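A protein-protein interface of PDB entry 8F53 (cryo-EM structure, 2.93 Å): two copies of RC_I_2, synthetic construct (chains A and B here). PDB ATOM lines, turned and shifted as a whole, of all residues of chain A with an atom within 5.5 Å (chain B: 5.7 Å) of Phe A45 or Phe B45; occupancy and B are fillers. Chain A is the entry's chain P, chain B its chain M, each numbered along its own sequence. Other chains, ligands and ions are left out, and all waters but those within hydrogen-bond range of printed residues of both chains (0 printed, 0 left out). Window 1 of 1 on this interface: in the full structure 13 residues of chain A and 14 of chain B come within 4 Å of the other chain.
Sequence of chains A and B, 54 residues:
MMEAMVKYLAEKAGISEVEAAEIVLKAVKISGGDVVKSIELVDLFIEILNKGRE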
ATOM      1  N   LEU A   9      16.475  -9.192  22.164  1.00  0.00           N
ATOM      2  CA  LEU A   9      17.699  -9.515  21.439  1.00  0.00           C
ATOM      3  C   LEU A   9      17.722  -8.851  20.066  1.00  0.00           C
ATOM      4  O   LEU A   9      18.752  -8.305  19.654  1.00  0.00           O
ATOM      5  CB  LEU A   9      17.835 -11.031  21.306  1.00  0.00           C
ATOM      6  CG  LEU A   9      19.073 -11.558  20.576  1.00  0.00           C
ATOM      7  CD1 LEU A   9      20.341 -11.140  21.287  1.00  0.00           C
ATOM      8  CD2 LEU A   9      19.013 -13.070  20.446  1.00  0.00           C
ATOM      9  N   ILE A  23      18.269 -17.900  17.743  1.00  0.00           N
ATOM     10  CA  ILE A  23      19.265 -17.812  18.808  1.00  0.00           C
ATOM     11  C   ILE A  23      18.612 -18.010  20.172  1.00  0.00           C
ATOM     12  O   ILE A  23      19.180 -18.657  21.061  1.00  0.00           O
ATOM     13  CB  ILE A  23      20.023 -16.475  18.724  1.00  0.00           C
ATOM     14  CG1 ILE A  23      20.845 -16.420  17.434  1.00  0.00           C
ATOM     15  CG2 ILE A  23      20.926 -16.311  19.928  1.00  0.00           C
ATOM     16  CD1 ILE A  23      21.486 -15.078  17.158  1.00  0.00           C
ATOM     17  N   LYS A  26      18.012 -21.653  20.673  1.00  0.00           N
ATOM     18  CA  LYS A  26      19.272 -22.275  21.070  1.00  0.00           C
ATOM     19  C   LYS A  26      19.544 -22.055  22.554  1.00  0.00           C
ATOM     20  O   LYS A  26      19.913 -22.988  23.279  1.00  0.00           O
ATOM     21  CB  LYS A  26      20.417 -21.708  20.231  1.00  0.00           C
ATOM     22  CG  LYS A  26      20.357 -22.057  18.758  1.00  0.00           C
ATOM     23  CD  LYS A  26      20.813 -23.476  18.508  1.00  0.00           C
ATOM     24  CE  LYS A  26      20.852 -23.783  17.024  1.00  0.00           C
ATOM     25  NZ  LYS A  26      21.864 -22.963  16.306  1.00  0.00           N
ATOM     26  N   ALA A  27      19.367 -20.818  23.022  1.00  0.00           N
ATOM     27  CA  ALA A  27      19.614 -20.508  24.428  1.00  0.00           C
ATOM     28  C   ALA A  27      18.681 -21.297  25.337  1.00  0.00           C
ATOM     29  O   ALA A  27      19.108 -21.847  26.357  1.00  0.00           O
ATOM     30  CB  ALA A  27      19.456 -19.007  24.670  1.00  0.00           C
ATOM     31  N   GLU A  40      20.207 -14.877  31.299  1.00  0.00           N
ATOM     32  CA  GLU A  40      21.645 -14.662  31.443  1.00  0.00           C
ATOM     33  C   GLU A  40      22.379 -14.975  30.147  1.00  0.00           C
ATOM     34  O   GLU A  40      23.264 -14.224  29.724  1.00  0.00           O
ATOM     35  CB  GLU A  40      22.197 -15.529  32.574  1.00  0.00           C
ATOM     36  CG  GLU A  40      21.618 -15.228  33.940  1.00  0.00           C
ATOM     37  CD  GLU A  40      22.033 -16.249  34.981  1.00  0.00           C
ATOM     38  OE1 GLU A  40      22.870 -17.118  34.663  1.00  0.00           O
ATOM     39  OE2 GLU A  40      21.519 -16.184  36.117  1.00  0.00           O
ATOM     40  N   LEU A  41      22.017 -16.082  29.498  1.00  0.00           N
ATOM     41  CA  LEU A  41      22.715 -16.501  28.289  1.00  0.00           C
ATOM     42  C   LEU A  41      22.395 -15.583  27.115  1.00  0.00           C
ATOM     43  O   LEU A  41      23.268 -15.299  26.289  1.00  0.00           O
ATOM     44  CB  LEU A  41      22.350 -17.950  27.972  1.00  0.00           C
ATOM     45  CG  LEU A  41      23.074 -18.649  26.824  1.00  0.00           C
ATOM     46  CD1 LEU A  41      24.572 -18.449  26.908  1.00  0.00           C
ATOM     47  CD2 LEU A  41      22.743 -20.127  26.837  1.00  0.00           C
ATOM     48  N   VAL A  42      21.152 -15.107  27.022  1.00  0.00           N
ATOM     49  CA  VAL A  42      20.805 -14.156  25.972  1.00  0.00           C
ATOM     50  C   VAL A  42      21.533 -12.837  26.181  1.00  0.00           C
ATOM     51  O   VAL A  42      21.923 -12.177  25.212  1.00  0.00           O
ATOM     52  CB  VAL A  42      19.281 -13.950  25.916  1.00  0.00           C
ATOM     53  CG1 VAL A  42      18.945 -12.768  25.025  1.00  0.00           C
ATOM     54  CG2 VAL A  42      18.595 -15.207  25.412  1.00  0.00           C
ATOM     55  N   ASP A  43      21.714 -12.417  27.435  1.00  0.00           N
ATOM     56  CA  ASP A  43      22.554 -11.253  27.703  1.00  0.00           C
ATOM     57  C   ASP A  43      23.992 -11.518  27.281  1.00  0.00           C
ATOM     58  O   ASP A  43      24.656 -10.640  26.717  1.00  0.00           O
ATOM     59  CB  ASP A  43      22.489 -10.885  29.183  1.00  0.00           C
ATOM     60  CG  ASP A  43      21.145 -10.315  29.581  1.00  0.00           C
ATOM     61  OD1 ASP A  43      20.473  -9.714  28.716  1.00  0.00           O
ATOM     62  OD2 ASP A  43      20.759 -10.465  30.760  1.00  0.00           O
ATOM     63  N   LEU A  44      24.494 -12.724  27.554  1.00  0.00           N
ATOM     64  CA  LEU A  44      25.845 -13.081  27.136  1.00  0.00           C
ATOM     65  C   LEU A  44      25.985 -13.030  25.618  1.00  0.00           C
ATOM     66  O   LEU A  44      27.022 -12.603  25.099  1.00  0.00           O
ATOM     67  CB  LEU A  44      26.199 -14.470  27.668  1.00  0.00           C
ATOM     68  CG  LEU A  44      27.587 -15.035  27.363  1.00  0.00           C
ATOM     69  CD1 LEU A  44      28.664 -14.024  27.684  1.00  0.00           C
ATOM     70  CD2 LEU A  44      27.816 -16.316  28.148  1.00  0.00           C
ATOM     71  N   PHE A  45      24.953 -13.460  24.887  1.00  0.00           N
ATOM     72  CA  PHE A  45      25.015 -13.416  23.429  1.00  0.00           C
ATOM     73  C   PHE A  45      25.118 -11.982  22.923  1.00  0.00           C
ATOM     74  O   PHE A  45      25.816 -11.712  21.940  1.00  0.00           O
ATOM     75  CB  PHE A  45      23.785 -14.090  22.815  1.00  0.00           C
ATOM     76  CG  PHE A  45      23.727 -15.587  22.999  1.00  0.00           C
ATOM     77  CD1 PHE A  45      24.845 -16.325  23.350  1.00  0.00           C
ATOM     78  CD2 PHE A  45      22.532 -16.257  22.800  1.00  0.00           C
ATOM     79  CE1 PHE A  45      24.765 -17.699  23.508  1.00  0.00           C
ATOM     80  CE2 PHE A  45      22.446 -17.626  22.954  1.00  0.00           C
ATOM     81  CZ  PHE A  45      23.563 -18.349  23.308  1.00  0.00           C
ATOM     82  N   ILE A  46      24.409 -11.052  23.567  1.00  0.00           N
ATOM     83  CA  ILE A  46      24.435  -9.660  23.127  1.00  0.00           C
ATOM     84  C   ILE A  46      25.844  -9.092  23.225  1.00  0.00           C
ATOM     85  O   ILE A  46      26.259  -8.292  22.378  1.00  0.00           O
ATOM     86  CB  ILE A  46      23.423  -8.827  23.940  1.00  0.00           C
ATOM     87  CG1 ILE A  46      21.996  -9.213  23.545  1.00  0.00           C
ATOM     88  CG2 ILE A  46      23.658  -7.340  23.723  1.00  0.00           C
ATOM     89  CD1 ILE A  46      20.923  -8.732  24.497  1.00  0.00           C
ATOM     90  N   GLU A  47      26.595  -9.476  24.257  1.00  0.00           N
ATOM     91  CA  GLU A  47      27.999  -9.088  24.341  1.00  0.00           C
ATOM     92  C   GLU A  47      28.801  -9.696  23.196  1.00  0.00           C
ATOM     93  O   GLU A  47      29.453  -8.985  22.425  1.00  0.00           O
ATOM     94  CB  GLU A  47      28.578  -9.515  25.689  1.00  0.00           C
ATOM     95  CG  GLU A  47      27.829  -8.966  26.887  1.00  0.00           C
ATOM     96  CD  GLU A  47      28.343  -9.531  28.195  1.00  0.00           C
ATOM     97  OE1 GLU A  47      29.448 -10.111  28.196  1.00  0.00           O
ATOM     98  OE2 GLU A  47      27.640  -9.403  29.221  1.00  0.00           O
ATOM     99  N   ILE A  48      28.748 -11.024  23.064  1.00  0.00           N
ATOM    100  CA  ILE A  48      29.521 -11.708  22.030  1.00  0.00           C
ATOM    101  C   ILE A  48      29.114 -11.213  20.649  1.00  0.00           C
ATOM    102  O   ILE A  48      29.960 -10.936  19.792  1.00  0.00           O
ATOM    103  CB  ILE A  48      29.340 -13.232  22.150  1.00  0.00           C
ATOM    104  CG1 ILE A  48      29.934 -13.738  23.467  1.00  0.00           C
ATOM    105  CG2 ILE A  48      29.979 -13.938  20.967  1.00  0.00           C
ATOM    106  CD1 ILE A  48      29.523 -15.151  23.825  1.00  0.00           C
ATOM    107  N   LEU A  49      27.809 -11.093  20.413  1.00  0.00           N
ATOM    108  CA  LEU A  49      27.319 -10.754  19.084  1.00  0.00           C
ATOM    109  C   LEU A  49      27.643  -9.322  18.682  1.00  0.00           C
ATOM    110  O   LEU A  49      27.518  -8.990  17.499  1.00  0.00           O
ATOM    111  CB  LEU A  49      25.807 -10.986  19.017  1.00  0.00           C
ATOM    112  CG  LEU A  49      25.130 -10.946  17.644  1.00  0.00           C
ATOM    113  CD1 LEU A  49      25.930 -11.703  16.600  1.00  0.00           C
ATOM    114  CD2 LEU A  49      23.729 -11.522  17.743  1.00  0.00           C
ATOM    115  N   ASN A  50      28.050  -8.470  19.624  1.00  0.00           N
ATOM    116  CA  ASN A  50      28.457  -7.103  19.313  1.00  0.00           C
ATOM    117  C   ASN A  50      29.969  -6.985  19.138  1.00  0.00           C
ATOM    118  O   ASN A  50      30.444  -6.567  18.078  1.00  0.00           O
ATOM    119  CB  ASN A  50      27.973  -6.143  20.409  1.00  0.00           C
ATOM    120  CG  ASN A  50      26.568  -5.629  20.155  1.00  0.00           C
ATOM    121  OD1 ASN A  50      26.361  -4.728  19.343  1.00  0.00           O
ATOM    122  ND2 ASN A  50      25.596  -6.192  20.860  1.00  0.00           N
ATOM    123  N   LEU B   9      38.697 -22.777  20.563  1.00  0.00           N
ATOM    124  CA  LEU B   9      37.901 -21.608  20.210  1.00  0.00           C
ATOM    125  C   LEU B   9      38.723 -20.592  19.424  1.00  0.00           C
ATOM    126  O   LEU B   9      38.239 -20.028  18.436  1.00  0.00           O
ATOM    127  CB  LEU B   9      37.324 -20.972  21.474  1.00  0.00           C
ATOM    128  CG  LEU B   9      36.520 -19.683  21.293  1.00  0.00           C
ATOM    129  CD1 LEU B   9      35.352 -19.898  20.353  1.00  0.00           C
ATOM    130  CD2 LEU B   9      36.027 -19.167  22.636  1.00  0.00           C
ATOM    131  N   ILE B  23      36.127 -15.480  26.784  1.00  0.00           N
ATOM    132  CA  ILE B  23      34.856 -16.088  26.399  1.00  0.00           C
ATOM    133  C   ILE B  23      34.699 -17.461  27.044  1.00  0.00           C
ATOM    134  O   ILE B  23      33.601 -17.842  27.468  1.00  0.00           O
ATOM    135  CB  ILE B  23      34.741 -16.157  24.865  1.00  0.00           C
ATOM    136  CG1 ILE B  23      34.657 -14.743  24.283  1.00  0.00           C
ATOM    137  CG2 ILE B  23      33.519 -16.957  24.468  1.00  0.00           C
ATOM    138  CD1 ILE B  23      34.783 -14.678  22.777  1.00  0.00           C
ATOM    139  N   LYS B  26      33.668 -16.958  30.575  1.00  0.00           N
ATOM    140  CA  LYS B  26      32.236 -16.664  30.596  1.00  0.00           C
ATOM    141  C   LYS B  26      31.415 -17.944  30.488  1.00  0.00           C
ATOM    142  O   LYS B  26      30.457 -18.153  31.245  1.00  0.00           O
ATOM    143  CB  LYS B  26      31.888 -15.713  29.451  1.00  0.00           C
ATOM    144  CG  LYS B  26      32.517 -14.336  29.555  1.00  0.00           C
ATOM    145  CD  LYS B  26      31.747 -13.444  30.501  1.00  0.00           C
ATOM    146  CE  LYS B  26      32.308 -12.035  30.494  1.00  0.00           C
ATOM    147  NZ  LYS B  26      32.135 -11.361  29.178  1.00  0.00           N
ATOM    148  N   ALA B  27      31.774 -18.810  29.537  1.00  0.00           N
ATOM    149  CA  ALA B  27      31.033 -20.053  29.344  1.00  0.00           C
ATOM    150  C   ALA B  27      31.109 -20.942  30.580  1.00  0.00           C
ATOM    151  O   ALA B  27      30.102 -21.517  31.002  1.00  0.00           O
ATOM    152  CB  ALA B  27      31.565 -20.795  28.118  1.00  0.00           C
ATOM    153  N   ILE B  30      28.923 -19.395  33.440  1.00  0.00           N
ATOM    154  CA  ILE B  30      27.479 -19.514  33.248  1.00  0.00           C
ATOM    155  C   ILE B  30      27.042 -20.977  33.256  1.00  0.00           C
ATOM    156  O   ILE B  30      25.899 -21.286  33.614  1.00  0.00           O
ATOM    157  CB  ILE B  30      27.053 -18.795  31.954  1.00  0.00           C
ATOM    158  CG1 ILE B  30      25.544 -18.558  31.941  1.00  0.00           C
ATOM    159  CG2 ILE B  30      27.448 -19.596  30.736  1.00  0.00           C
ATOM    160  CD1 ILE B  30      25.104 -17.522  30.936  1.00  0.00           C
ATOM    161  N   GLU B  40      29.425 -27.528  25.072  1.00  0.00           N
ATOM    162  CA  GLU B  40      28.265 -27.208  24.246  1.00  0.00           C
ATOM    163  C   GLU B  40      28.158 -25.708  24.002  1.00  0.00           C
ATOM    164  O   GLU B  40      27.898 -25.271  22.876  1.00  0.00           O
ATOM    165  CB  GLU B  40      26.992 -27.728  24.911  1.00  0.00           C
ATOM    166  CG  GLU B  40      26.931 -29.236  25.031  1.00  0.00           C
ATOM    167  CD  GLU B  40      25.757 -29.705  25.866  1.00  0.00           C
ATOM    168  OE1 GLU B  40      24.951 -28.854  26.295  1.00  0.00           O
ATOM    169  OE2 GLU B  40      25.640 -30.926  26.097  1.00  0.00           O
ATOM    170  N   LEU B  41      28.356 -24.902  25.048  1.00  0.00           N
ATOM    171  CA  LEU B  41      28.286 -23.453  24.897  1.00  0.00           C
ATOM    172  C   LEU B  41      29.400 -22.933  23.998  1.00  0.00           C
ATOM    173  O   LEU B  41      29.163 -22.074  23.142  1.00  0.00           O
ATOM    174  CB  LEU B  41      28.352 -22.784  26.269  1.00  0.00           C
ATOM    175  CG  LEU B  41      27.011 -22.561  26.969  1.00  0.00           C
ATOM    176  CD1 LEU B  41      27.199 -22.406  28.466  1.00  0.00           C
ATOM    177  CD2 LEU B  41      26.330 -21.340  26.395  1.00  0.00           C
ATOM    178  N   VAL B  42      30.625 -23.433  24.177  1.00  0.00           N
ATOM    179  CA  VAL B  42      31.729 -22.977  23.339  1.00  0.00           C
ATOM    180  C   VAL B  42      31.478 -23.330  21.883  1.00  0.00           C
ATOM    181  O   VAL B  42      31.829 -22.561  20.982  1.00  0.00           O
ATOM    182  CB  VAL B  42      33.060 -23.568  23.839  1.00  0.00           C
ATOM    183  CG1 VAL B  42      34.160 -23.318  22.826  1.00  0.00           C
ATOM    184  CG2 VAL B  42      33.427 -22.966  25.182  1.00  0.00           C
ATOM    185  N   ASP B  43      30.880 -24.494  21.623  1.00  0.00           N
ATOM    186  CA  ASP B  43      30.466 -24.818  20.260  1.00  0.00           C
ATOM    187  C   ASP B  43      29.400 -23.844  19.774  1.00  0.00           C
ATOM    188  O   ASP B  43      29.432 -23.392  18.624  1.00  0.00           O
ATOM    189  CB  ASP B  43      29.947 -26.253  20.197  1.00  0.00           C
ATOM    190  CG  ASP B  43      31.054 -27.278  20.328  1.00  0.00           C
ATOM    191  OD1 ASP B  43      32.202 -26.967  19.943  1.00  0.00           O
ATOM    192  OD2 ASP B  43      30.778 -28.395  20.814  1.00  0.00           O
ATOM    193  N   LEU B  44      28.443 -23.512  20.641  1.00  0.00           N
ATOM    194  CA  LEU B  44      27.398 -22.563  20.270  1.00  0.00           C
ATOM    195  C   LEU B  44      27.981 -21.188  19.968  1.00  0.00           C
ATOM    196  O   LEU B  44      27.516 -20.498  19.054  1.00  0.00           O
ATOM    197  CB  LEU B  44      26.356 -22.481  21.387  1.00  0.00           C
ATOM    198  CG  LEU B  44      25.145 -21.568  21.186  1.00  0.00           C
ATOM    199  CD1 LEU B  44      24.477 -21.832  19.854  1.00  0.00           C
ATOM    200  CD2 LEU B  44      24.149 -21.756  22.319  1.00  0.00           C
ATOM    201  N   PHE B  45      28.998 -20.767  20.727  1.00  0.00           N
ATOM    202  CA  PHE B  45      29.632 -19.480  20.456  1.00  0.00           C
ATOM    203  C   PHE B  45      30.311 -19.475  19.094  1.00  0.00           C
ATOM    204  O   PHE B  45      30.315 -18.453  18.399  1.00  0.00           O
ATOM    205  CB  PHE B  45      30.657 -19.143  21.543  1.00  0.00           C
ATOM    206  CG  PHE B  45      30.067 -18.883  22.908  1.00  0.00           C
ATOM    207  CD1 PHE B  45      28.714 -18.644  23.084  1.00  0.00           C
ATOM    208  CD2 PHE B  45      30.890 -18.869  24.020  1.00  0.00           C
ATOM    209  CE1 PHE B  45      28.198 -18.404  24.348  1.00  0.00           C
ATOM    210  CE2 PHE B  45      30.381 -18.630  25.282  1.00  0.00           C
ATOM    211  CZ  PHE B  45      29.034 -18.397  25.447  1.00  0.00           C
ATOM    212  N   ILE B  46      30.907 -20.603  18.699  1.00  0.00           N
ATOM    213  CA  ILE B  46      31.587 -20.674  17.408  1.00  0.00           C
ATOM    214  C   ILE B  46      30.601 -20.445  16.273  1.00  0.00           C
ATOM    215  O   ILE B  46      30.950 -19.850  15.246  1.00  0.00           O
ATOM    216  CB  ILE B  46      32.319 -22.025  17.271  1.00  0.00           C
ATOM    217  CG1 ILE B  46      33.552 -22.043  18.178  1.00  0.00           C
ATOM    218  CG2 ILE B  46      32.712 -22.276  15.822  1.00  0.00           C
ATOM    219  CD1 ILE B  46      34.155 -23.410  18.397  1.00  0.00           C
ATOM    220  N   GLU B  47      29.364 -20.919  16.425  1.00  0.00           N
ATOM    221  CA  GLU B  47      28.326 -20.610  15.448  1.00  0.00           C
ATOM    222  C   GLU B  47      27.980 -19.125  15.475  1.00  0.00           C
ATOM    223  O   GLU B  47      28.052 -18.437  14.450  1.00  0.00           O
ATOM    224  CB  GLU B  47      27.083 -21.455  15.727  1.00  0.00           C
ATOM    225  CG  GLU B  47      27.341 -22.948  15.749  1.00  0.00           C
ATOM    226  CD  GLU B  47      26.125 -23.736  16.189  1.00  0.00           C
ATOM    227  OE1 GLU B  47      25.016 -23.162  16.191  1.00  0.00           O
ATOM    228  OE2 GLU B  47      26.277 -24.924  16.542  1.00  0.00           O
ATOM    229  N   ILE B  48      27.617 -18.610  16.651  1.00  0.00           N
ATOM    230  CA  ILE B  48      27.237 -17.205  16.773  1.00  0.00           C
ATOM    231  C   ILE B  48      28.391 -16.306  16.346  1.00  0.00           C
ATOM    232  O   ILE B  48      28.204 -15.335  15.603  1.00  0.00           O
ATOM    233  CB  ILE B  48      26.794 -16.895  18.214  1.00  0.00           C
ATOM    234  CG1 ILE B  48      25.513 -17.660  18.556  1.00  0.00           C
ATOM    235  CG2 ILE B  48      26.591 -15.403  18.398  1.00  0.00           C
ATOM    236  CD1 ILE B  48      25.197 -17.696  20.035  1.00  0.00           C
ATOM    237  N   LEU B  49      29.601 -16.617  16.807  1.00  0.00           N
ATOM    238  CA  LEU B  49      30.738 -15.739  16.571  1.00  0.00           C
ATOM    239  C   LEU B  49      31.197 -15.745  15.120  1.00  0.00           C
ATOM    240  O   LEU B  49      32.003 -14.885  14.745  1.00  0.00           O
ATOM    241  CB  LEU B  49      31.898 -16.143  17.485  1.00  0.00           C
ATOM    242  CG  LEU B  49      33.107 -15.208  17.575  1.00  0.00           C
ATOM    243  CD1 LEU B  49      32.689 -13.752  17.683  1.00  0.00           C
ATOM    244  CD2 LEU B  49      33.966 -15.591  18.768  1.00  0.00           C
ATOM    245  N   ASN B  50      30.715 -16.677  14.298  1.00  0.00           N
ATOM    246  CA  ASN B  50      31.033 -16.698  12.873  1.00  0.00           C
ATOM    247  C   ASN B  50      29.919 -16.079  12.035  1.00  0.00           C
ATOM    248  O   ASN B  50      30.156 -15.123  11.291  1.00  0.00           O
ATOM    249  CB  ASN B  50      31.307 -18.136  12.410  1.00  0.00           C
ATOM    250  CG  ASN B  50      32.746 -18.561  12.640  1.00  0.00           C
ATOM    251  OD1 ASN B  50      33.660 -18.091  11.964  1.00  0.00           O
ATOM    252  ND2 ASN B  50      32.951 -19.467  13.589  1.00  0.00           N
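Among the printed residues, merely in contact across the chains: Glu A40 with Ile B30, Leu A41 with Ile B30, Leu A41 with Leu B41, Leu A44 with Phe B45, Phe A45 with Leu B44, Phe A45 with Phe B45, Phe A45 with Ile B48 and Ile A48 with Phe B45.
Printed residues of chain B within 4 Å of Phe A45: Leu B44 (3.6 Å), Phe B45 (3.6 Å) and Ile B48 (3.5 Å).
Of the printed residues of chain A, Leu B44 touches Phe A45 (3.6 Å).
Of the printed residues of chain A, Glu B47 touches Lys A26.
Leu A49 touches none of the printed residues of chain B.
Ile A46 touches none of the printed residues of chain B.
The nearest residue of chain A that does not touch Phe B45 is Leu A41 (4.4 Å).
The nearest printed residue of chain A that does not touch Leu B41 is Phe A45 (4.9 Å).
The side-chain amino group (NZ) of Lys B26 is in salt-bridge range of the side-chain carboxylate (OE1) of Glu A47.
OE1 of Glu B47 lies within salt-bridge range of NZ of Lys A26, at 3.2 Å.
Lys A26 touches Glu B47, and with the chains exchanged Glu A47 touches Lys B26.
Leu A44 touches Phe B45, and with the chains exchanged Phe A45 touches Leu B44.
Phe B45 touches its own counterpart, Phe A45.
Phe A45 touches Ile B48, and with the chains exchanged Ile A48 touches Phe B45.
Of the 15 printed residues of chain A, 7 touch a printed residue of chain B.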
